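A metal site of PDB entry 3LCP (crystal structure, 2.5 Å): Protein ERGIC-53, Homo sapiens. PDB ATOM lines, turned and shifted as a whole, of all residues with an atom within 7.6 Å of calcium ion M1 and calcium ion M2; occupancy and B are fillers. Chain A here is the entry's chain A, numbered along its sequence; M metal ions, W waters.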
ATOM      1  N   ASP A  91     -15.293  -1.150  -9.622  1.00  0.00           N
ATOM      2  CA  ASP A  91     -15.398  -2.546  -9.193  1.00  0.00           C
ATOM      3  C   ASP A  91     -16.773  -2.859  -8.702  1.00  0.00           C
ATOM      4  O   ASP A  91     -17.287  -3.971  -8.911  1.00  0.00           O
ATOM      5  CB  ASP A  91     -14.430  -2.802  -8.014  1.00  0.00           C
ATOM      6  CG  ASP A  91     -13.028  -3.159  -8.492  1.00  0.00           C
ATOM      7  OD1 ASP A  91     -12.908  -4.038  -9.366  1.00  0.00           O
ATOM      8  OD2 ASP A  91     -12.063  -2.543  -8.003  1.00  0.00           O
ATOM      9  N   GLY A  92     -17.352  -1.887  -7.974  1.00  0.00           N
ATOM     10  CA  GLY A  92     -18.751  -1.960  -7.573  1.00  0.00           C
ATOM     11  C   GLY A  92     -19.024  -1.294  -6.255  1.00  0.00           C
ATOM     12  O   GLY A  92     -18.190  -0.562  -5.716  1.00  0.00           O
ATOM     13  N   PHE A 108     -14.507  -3.825  -1.594  1.00  0.00           N
ATOM     14  CA  PHE A 108     -15.291  -2.791  -2.234  1.00  0.00           C
ATOM     15  C   PHE A 108     -15.185  -1.488  -1.488  1.00  0.00           C
ATOM     16  O   PHE A 108     -16.203  -0.795  -1.305  1.00  0.00           O
ATOM     17  CB  PHE A 108     -16.778  -3.196  -2.352  1.00  0.00           C
ATOM     18  CG  PHE A 108     -17.027  -4.240  -3.364  1.00  0.00           C
ATOM     19  CD1 PHE A 108     -17.330  -3.879  -4.678  1.00  0.00           C
ATOM     20  CD2 PHE A 108     -16.921  -5.594  -3.046  1.00  0.00           C
ATOM     21  CE1 PHE A 108     -17.534  -4.837  -5.643  1.00  0.00           C
ATOM     22  CE2 PHE A 108     -17.141  -6.558  -3.994  1.00  0.00           C
ATOM     23  CZ  PHE A 108     -17.439  -6.176  -5.301  1.00  0.00           C
ATOM     24  N   PHE A 121     -22.809  -5.218  -4.937  1.00  0.00           N
ATOM     25  CA  PHE A 121     -23.278  -4.939  -6.246  1.00  0.00           C
ATOM     26  C   PHE A 121     -22.016  -4.997  -7.125  1.00  0.00           C
ATOM     27  O   PHE A 121     -21.260  -4.016  -7.203  1.00  0.00           O
ATOM     28  CB  PHE A 121     -23.971  -3.560  -6.231  1.00  0.00           C
ATOM     29  CG  PHE A 121     -25.229  -3.553  -5.421  1.00  0.00           C
ATOM     30  CD1 PHE A 121     -25.176  -3.547  -4.054  1.00  0.00           C
ATOM     31  CD2 PHE A 121     -26.459  -3.587  -6.042  1.00  0.00           C
ATOM     32  CE1 PHE A 121     -26.320  -3.542  -3.282  1.00  0.00           C
ATOM     33  CE2 PHE A 121     -27.621  -3.619  -5.313  1.00  0.00           C
ATOM     34  CZ  PHE A 121     -27.535  -3.585  -3.886  1.00  0.00           C
ATOM     35  N   ASP A 122     -21.783  -6.171  -7.717  1.00  0.00           N
ATOM     36  CA  ASP A 122     -20.480  -6.491  -8.316  1.00  0.00           C
ATOM     37  C   ASP A 122     -20.559  -6.297  -9.831  1.00  0.00           C
ATOM     38  O   ASP A 122     -21.200  -7.049 -10.549  1.00  0.00           O
ATOM     39  CB  ASP A 122     -20.038  -7.922  -7.983  1.00  0.00           C
ATOM     40  CG  ASP A 122     -18.537  -8.174  -8.222  1.00  0.00           C
ATOM     41  OD1 ASP A 122     -17.931  -8.923  -7.446  1.00  0.00           O
ATOM     42  OD2 ASP A 122     -17.946  -7.651  -9.180  1.00  0.00           O
ATOM     43  N   SER A 123     -19.918  -5.249 -10.285  1.00  0.00           N
ATOM     44  CA  SER A 123     -19.953  -4.973 -11.720  1.00  0.00           C
ATOM     45  C   SER A 123     -18.769  -5.603 -12.457  1.00  0.00           C
ATOM     46  O   SER A 123     -18.818  -5.746 -13.667  1.00  0.00           O
ATOM     47  CB  SER A 123     -20.036  -3.464 -11.951  1.00  0.00           C
ATOM     48  OG  SER A 123     -18.916  -2.833 -11.378  1.00  0.00           O
ATOM     49  N   PHE A 124     -17.733  -6.047 -11.722  1.00  0.00           N
ATOM     50  CA  PHE A 124     -16.537  -6.609 -12.410  1.00  0.00           C
ATOM     51  C   PHE A 124     -16.307  -8.127 -12.312  1.00  0.00           C
ATOM     52  O   PHE A 124     -16.258  -8.693 -11.224  1.00  0.00           O
ATOM     53  CB  PHE A 124     -15.268  -5.832 -12.079  1.00  0.00           C
ATOM     54  CG  PHE A 124     -14.090  -6.209 -12.947  1.00  0.00           C
ATOM     55  CD1 PHE A 124     -14.028  -5.787 -14.265  1.00  0.00           C
ATOM     56  CD2 PHE A 124     -13.067  -6.993 -12.435  1.00  0.00           C
ATOM     57  CE1 PHE A 124     -12.934  -6.141 -15.076  1.00  0.00           C
ATOM     58  CE2 PHE A 124     -11.968  -7.373 -13.223  1.00  0.00           C
ATOM     59  CZ  PHE A 124     -11.897  -6.942 -14.545  1.00  0.00           C
ATOM     60  N   ASP A 125     -16.193  -8.768 -13.473  1.00  0.00           N
ATOM     61  CA  ASP A 125     -16.199 -10.219 -13.603  1.00  0.00           C
ATOM     62  C   ASP A 125     -14.772 -10.744 -13.362  1.00  0.00           C
ATOM     63  O   ASP A 125     -13.955 -10.897 -14.279  1.00  0.00           O
ATOM     64  CB  ASP A 125     -16.776 -10.607 -14.993  1.00  0.00           C
ATOM     65  CG  ASP A 125     -16.953 -12.108 -15.175  1.00  0.00           C
ATOM     66  OD1 ASP A 125     -16.816 -12.881 -14.204  1.00  0.00           O
ATOM     67  OD2 ASP A 125     -17.289 -12.536 -16.299  1.00  0.00           O
ATOM     68  N   ASN A 126     -14.433 -10.966 -12.113  1.00  0.00           N
ATOM     69  CA  ASN A 126     -13.053 -11.244 -11.806  1.00  0.00           C
ATOM     70  C   ASN A 126     -12.670 -12.659 -12.148  1.00  0.00           C
ATOM     71  O   ASN A 126     -11.534 -12.891 -12.511  1.00  0.00           O
ATOM     72  CB  ASN A 126     -12.735 -10.903 -10.354  1.00  0.00           C
ATOM     73  CG  ASN A 126     -12.520  -9.454 -10.167  1.00  0.00           C
ATOM     74  OD1 ASN A 126     -13.442  -8.706  -9.801  1.00  0.00           O
ATOM     75  ND2 ASN A 126     -11.301  -9.015 -10.431  1.00  0.00           N
ATOM     76  N   ASP A 127     -13.622 -13.585 -12.043  1.00  0.00           N
ATOM     77  CA  ASP A 127     -13.407 -15.001 -12.381  1.00  0.00           C
ATOM     78  C   ASP A 127     -13.813 -15.387 -13.829  1.00  0.00           C
ATOM     79  O   ASP A 127     -13.833 -16.589 -14.182  1.00  0.00           O
ATOM     80  CB  ASP A 127     -14.161 -15.903 -11.377  1.00  0.00           C
ATOM     81  CG  ASP A 127     -15.650 -15.555 -11.294  1.00  0.00           C
ATOM     82  OD1 ASP A 127     -16.116 -14.634 -12.025  1.00  0.00           O
ATOM     83  OD2 ASP A 127     -16.381 -16.233 -10.522  1.00  0.00           O
ATOM     84  N   GLY A 128     -14.135 -14.389 -14.663  1.00  0.00           N
ATOM     85  CA  GLY A 128     -14.459 -14.621 -16.075  1.00  0.00           C
ATOM     86  C   GLY A 128     -15.589 -15.587 -16.341  1.00  0.00           C
ATOM     87  O   GLY A 128     -15.643 -16.234 -17.402  1.00  0.00           O
ATOM     88  N   LYS A 129     -16.515 -15.696 -15.382  1.00  0.00           N
ATOM     89  CA  LYS A 129     -17.659 -16.609 -15.512  1.00  0.00           C
ATOM     90  C   LYS A 129     -18.833 -16.023 -16.296  1.00  0.00           C
ATOM     91  O   LYS A 129     -19.886 -16.653 -16.402  1.00  0.00           O
ATOM     92  CB  LYS A 129     -18.120 -17.101 -14.134  1.00  0.00           C
ATOM     93  CG  LYS A 129     -17.170 -18.116 -13.510  1.00  0.00           C
ATOM     94  CD  LYS A 129     -17.940 -19.297 -12.919  1.00  0.00           C
ATOM     95  CE  LYS A 129     -17.188 -20.616 -13.166  1.00  0.00           C
ATOM     96  NZ  LYS A 129     -15.741 -20.582 -12.788  1.00  0.00           N
ATOM     97  N   LYS A 130     -18.649 -14.813 -16.842  1.00  0.00           N
ATOM     98  CA  LYS A 130     -19.678 -14.131 -17.667  1.00  0.00           C
ATOM     99  C   LYS A 130     -20.982 -13.853 -16.891  1.00  0.00           C
ATOM    100  O   LYS A 130     -22.095 -13.946 -17.459  1.00  0.00           O
ATOM    101  CB  LYS A 130     -20.004 -14.913 -18.968  1.00  0.00           C
ATOM    102  CG  LYS A 130     -18.820 -15.486 -19.788  1.00  0.00           C
ATOM    103  CD  LYS A 130     -18.251 -14.480 -20.777  1.00  0.00           C
ATOM    104  CE  LYS A 130     -17.286 -15.180 -21.707  1.00  0.00           C
ATOM    105  NZ  LYS A 130     -16.939 -14.382 -22.921  1.00  0.00           N
ATOM    106  N   ASN A 131     -20.856 -13.548 -15.592  1.00  0.00           N
ATOM    107  CA  ASN A 131     -22.015 -13.462 -14.699  1.00  0.00           C
ATOM    108  C   ASN A 131     -22.009 -12.180 -13.863  1.00  0.00           C
ATOM    109  O   ASN A 131     -22.107 -12.226 -12.618  1.00  0.00           O
ATOM    110  CB  ASN A 131     -22.170 -14.735 -13.845  1.00  0.00           C
ATOM    111  CG  ASN A 131     -20.964 -15.012 -12.903  1.00  0.00           C
ATOM    112  OD1 ASN A 131     -19.890 -14.409 -13.014  1.00  0.00           O
ATOM    113  ND2 ASN A 131     -21.167 -15.933 -11.956  1.00  0.00           N
ATOM    114  N   ASN A 132     -21.885 -11.063 -14.567  1.00  0.00           N
ATOM    115  CA  ASN A 132     -21.795  -9.720 -14.013  1.00  0.00           C
ATOM    116  C   ASN A 132     -22.408  -8.735 -15.023  1.00  0.00           C
ATOM    117  O   ASN A 132     -22.511  -9.064 -16.209  1.00  0.00           O
ATOM    118  CB  ASN A 132     -20.349  -9.316 -13.794  1.00  0.00           C
ATOM    119  CG  ASN A 132     -19.643 -10.147 -12.742  1.00  0.00           C
ATOM    120  OD1 ASN A 132     -19.398 -11.347 -12.930  1.00  0.00           O
ATOM    121  ND2 ASN A 132     -19.231  -9.496 -11.654  1.00  0.00           N
ATOM    122  N   ALA A 134     -23.515  -8.299 -11.085  1.00  0.00           N
ATOM    123  CA  ALA A 134     -24.250  -9.223 -10.212  1.00  0.00           C
ATOM    124  C   ALA A 134     -24.422  -8.618  -8.856  1.00  0.00           C
ATOM    125  O   ALA A 134     -23.637  -7.758  -8.479  1.00  0.00           O
ATOM    126  CB  ALA A 134     -23.501 -10.550 -10.073  1.00  0.00           C
ATOM    127  N   TYR A 146     -12.872 -12.045   2.307  1.00  0.00           N
ATOM    128  CA  TYR A 146     -13.590 -11.920   1.030  1.00  0.00           C
ATOM    129  C   TYR A 146     -12.758 -12.468  -0.133  1.00  0.00           C
ATOM    130  O   TYR A 146     -11.596 -12.076  -0.329  1.00  0.00           O
ATOM    131  CB  TYR A 146     -13.990 -10.472   0.755  1.00  0.00           C
ATOM    132  CG  TYR A 146     -14.640 -10.281  -0.597  1.00  0.00           C
ATOM    133  CD1 TYR A 146     -15.854 -10.871  -0.889  1.00  0.00           C
ATOM    134  CD2 TYR A 146     -14.047  -9.478  -1.575  1.00  0.00           C
ATOM    135  CE1 TYR A 146     -16.456 -10.703  -2.116  1.00  0.00           C
ATOM    136  CE2 TYR A 146     -14.642  -9.292  -2.818  1.00  0.00           C
ATOM    137  CZ  TYR A 146     -15.839  -9.919  -3.078  1.00  0.00           C
ATOM    138  OH  TYR A 146     -16.468  -9.776  -4.281  1.00  0.00           O
ATOM    139  N   ASP A 147     -13.331 -13.391  -0.882  1.00  0.00           N
ATOM    140  CA  ASP A 147     -12.656 -13.863  -2.066  1.00  0.00           C
ATOM    141  C   ASP A 147     -13.052 -13.037  -3.298  1.00  0.00           C
ATOM    142  O   ASP A 147     -14.032 -13.366  -3.962  1.00  0.00           O
ATOM    143  CB  ASP A 147     -12.978 -15.341  -2.277  1.00  0.00           C
ATOM    144  CG  ASP A 147     -12.233 -15.940  -3.467  1.00  0.00           C
ATOM    145  OD1 ASP A 147     -12.797 -16.838  -4.127  1.00  0.00           O
ATOM    146  OD2 ASP A 147     -11.098 -15.520  -3.753  1.00  0.00           O
ATOM    147  N   HIS A 148     -12.310 -11.981  -3.606  1.00  0.00           N
ATOM    148  CA  HIS A 148     -12.716 -11.096  -4.726  1.00  0.00           C
ATOM    149  C   HIS A 148     -12.359 -11.612  -6.094  1.00  0.00           C
ATOM    150  O   HIS A 148     -12.909 -11.093  -7.080  1.00  0.00           O
ATOM    151  CB  HIS A 148     -12.220  -9.611  -4.597  1.00  0.00           C
ATOM    152  CG  HIS A 148     -10.744  -9.518  -4.408  1.00  0.00           C
ATOM    153  ND1 HIS A 148      -9.994 -10.666  -4.423  1.00  0.00           N
ATOM    154  CD2 HIS A 148      -9.781  -8.574  -3.965  1.00  0.00           C
ATOM    155  CE1 HIS A 148      -8.689 -10.507  -4.132  1.00  0.00           C
ATOM    156  NE2 HIS A 148      -8.507  -9.259  -3.756  1.00  0.00           N
ATOM    157  N   GLN A 149     -11.468 -12.597  -6.181  1.00  0.00           N
ATOM    158  CA  GLN A 149     -11.056 -13.153  -7.466  1.00  0.00           C
ATOM    159  C   GLN A 149     -12.105 -14.107  -8.006  1.00  0.00           C
ATOM    160  O   GLN A 149     -12.123 -14.392  -9.206  1.00  0.00           O
ATOM    161  CB  GLN A 149      -9.691 -13.849  -7.361  1.00  0.00           C
ATOM    162  CG  GLN A 149      -8.505 -12.898  -7.112  1.00  0.00           C
ATOM    163  CD  GLN A 149      -8.398 -11.766  -8.164  1.00  0.00           C
ATOM    164  OE1 GLN A 149      -8.242 -10.591  -7.811  1.00  0.00           O
ATOM    165  NE2 GLN A 149      -8.448 -12.123  -9.439  1.00  0.00           N
ATOM    166  N   ASN A 150     -12.974 -14.589  -7.141  1.00  0.00           N
ATOM    167  CA  ASN A 150     -14.133 -15.341  -7.598  1.00  0.00           C
ATOM    168  C   ASN A 150     -15.451 -14.615  -7.372  1.00  0.00           C
ATOM    169  O   ASN A 150     -16.501 -15.238  -7.310  1.00  0.00           O
ATOM    170  CB  ASN A 150     -14.172 -16.729  -6.969  1.00  0.00           C
ATOM    171  CG  ASN A 150     -13.236 -17.724  -7.666  1.00  0.00           C
ATOM    172  OD1 ASN A 150     -12.672 -17.464  -8.748  1.00  0.00           O
ATOM    173  ND2 ASN A 150     -13.057 -18.878  -7.027  1.00  0.00           N
ATOM    174  N   ASP A 151     -15.381 -13.287  -7.235  1.00  0.00           N
ATOM    175  CA  ASP A 151     -16.589 -12.458  -7.030  1.00  0.00           C
ATOM    176  C   ASP A 151     -17.458 -13.020  -5.908  1.00  0.00           C
ATOM    177  O   ASP A 151     -18.682 -13.011  -6.005  1.00  0.00           O
ATOM    178  CB  ASP A 151     -17.433 -12.447  -8.301  1.00  0.00           C
ATOM    179  CG  ASP A 151     -16.781 -11.736  -9.456  1.00  0.00           C
ATOM    180  OD1 ASP A 151     -17.113 -12.191 -10.557  1.00  0.00           O
ATOM    181  OD2 ASP A 151     -16.047 -10.724  -9.286  1.00  0.00           O
ATOM    182  N   GLY A 152     -16.800 -13.582  -4.899  1.00  0.00           N
ATOM    183  CA  GLY A 152     -17.434 -14.136  -3.708  1.00  0.00           C
ATOM    184  C   GLY A 152     -18.280 -15.353  -3.928  1.00  0.00           C
ATOM    185  O   GLY A 152     -18.971 -15.806  -3.010  1.00  0.00           O
ATOM    186  N   ALA A 153     -18.202 -15.928  -5.129  1.00  0.00           N
ATOM    187  CA  ALA A 153     -18.977 -17.127  -5.461  1.00  0.00           C
ATOM    188  C   ALA A 153     -18.799 -18.322  -4.518  1.00  0.00           C
ATOM    189  O   ALA A 153     -19.647 -19.211  -4.464  1.00  0.00           O
ATOM    190  CB  ALA A 153     -18.709 -17.544  -6.877  1.00  0.00           C
ATOM    191  N   GLN A 161     -28.548 -11.694 -10.987  1.00  0.00           N
ATOM    192  CA  GLN A 161     -27.965 -10.973 -12.099  1.00  0.00           C
ATOM    193  C   GLN A 161     -28.784  -9.724 -12.363  1.00  0.00           C
ATOM    194  O   GLN A 161     -29.873  -9.830 -12.884  1.00  0.00           O
ATOM    195  CB  GLN A 161     -27.948 -11.867 -13.350  1.00  0.00           C
ATOM    196  CG  GLN A 161     -27.122 -13.172 -13.176  1.00  0.00           C
ATOM    197  CD  GLN A 161     -25.656 -12.960 -13.449  1.00  0.00           C
ATOM    198  OE1 GLN A 161     -25.265 -12.688 -14.581  1.00  0.00           O
ATOM    199  NE2 GLN A 161     -24.834 -13.060 -12.414  1.00  0.00           N
HETATM  200 CA    CA M   1     -15.572  -8.762  -8.793  1.00  0.00          CA
HETATM  201 CA    CA M   2     -18.196 -13.311 -12.128  1.00  0.00          CA
HETATM  202  O   HOH W   1     -15.121  -8.964  -6.326  1.00  0.00           O
HETATM  203  O   HOH W   2     -18.972 -15.084 -10.809  1.00  0.00           O
HETATM  204  O   HOH W   3     -20.318 -12.401 -10.664  1.00  0.00           O
HETATM  205  O   HOH W   4     -15.398  -6.490  -8.614  1.00  0.00           O
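Calcium ion M2 is bound by OD1 of Asn 131, OD1 of Asp 151, water W2, OD1 of Asn 132, OD1 of Asp 127, OD1 of Asp 125 and water W3. Calcium ion M2 has seven donor atoms within binding distance.
Water W1 lies within hydrogen-bond range of the side-chain hydroxyl (OH) of Tyr 146 (2.6 Å) and the backbone carbonyl oxygen (O) of His 148 (3.2 Å). Water W3 lies within hydrogen-bond range of the backbone carbonyl oxygen (O) of Asn 131 (2.7 Å) and the side-chain amide nitrogen (ND2) of Asn 132 (3.3 Å). Water W2 bridges the side-chain amide nitrogen of Asn 131 (2.6 Å) and the side-chain carboxylate of Asp 127 (2.8 Å).
His 148 touches calcium ion M1 (O to CA, 3.9 Å). Within 4 Å of calcium ion M1: Asp 122, Phe 124, Asn 126, His 148 and Asp 151. Along chain A the residues within 4 Å of calcium ion M1 span positions 122 to 151.
The side-chain carboxylate (OD1) of Asp 125 sits close to the backbone NH (N) of Gly 128 (3.1 Å). OD2 of Asp 125 lies within hydrogen-bond range of N of Lys 129, at 3.4 Å. The side-chain carboxylate (OD2) of Asp 125 lies within hydrogen-bond range of the backbone NH (N) of Lys 130. ND2 of Asn 132 is in hydrogen-bond range of O of Asp 122. O of Ala 134 sits at hydrogen-bond distance from N of Asp 122 (2.6 Å). The backbone carbonyl oxygen (O) of Gln 149 sits at hydrogen-bond distance from the backbone NH (N) of Asp 127. The backbone carbonyl oxygen (O) of Asn 131 is in hydrogen-bond range of the side-chain amide nitrogen (NE2) of Gln 161. ND2 of Asn 132 sits close to O of Phe 124 (3.1 Å).
Calcium ion M1 is bound by the side-chain carboxylate (OD2) of Asp 151 (2.1 Å), water W4 (2.3 Å), the side-chain amide oxygen (OD1) of Asn 126 (2.4 Å), water W1 (2.5 Å), the backbone carbonyl oxygen (O) of Phe 124 (2.5 Å), the side-chain carboxylate (OD2) of Asp 122 (2.6 Å) and the side-chain carboxylate (OD1) of Asp 122 (2.7 Å).
Of the 25 residues printed, 5 come within 4 Å of calcium ion M2. The nearest printed residue that does not touch calcium ion M2 is Lys 129 (4.3 Å).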
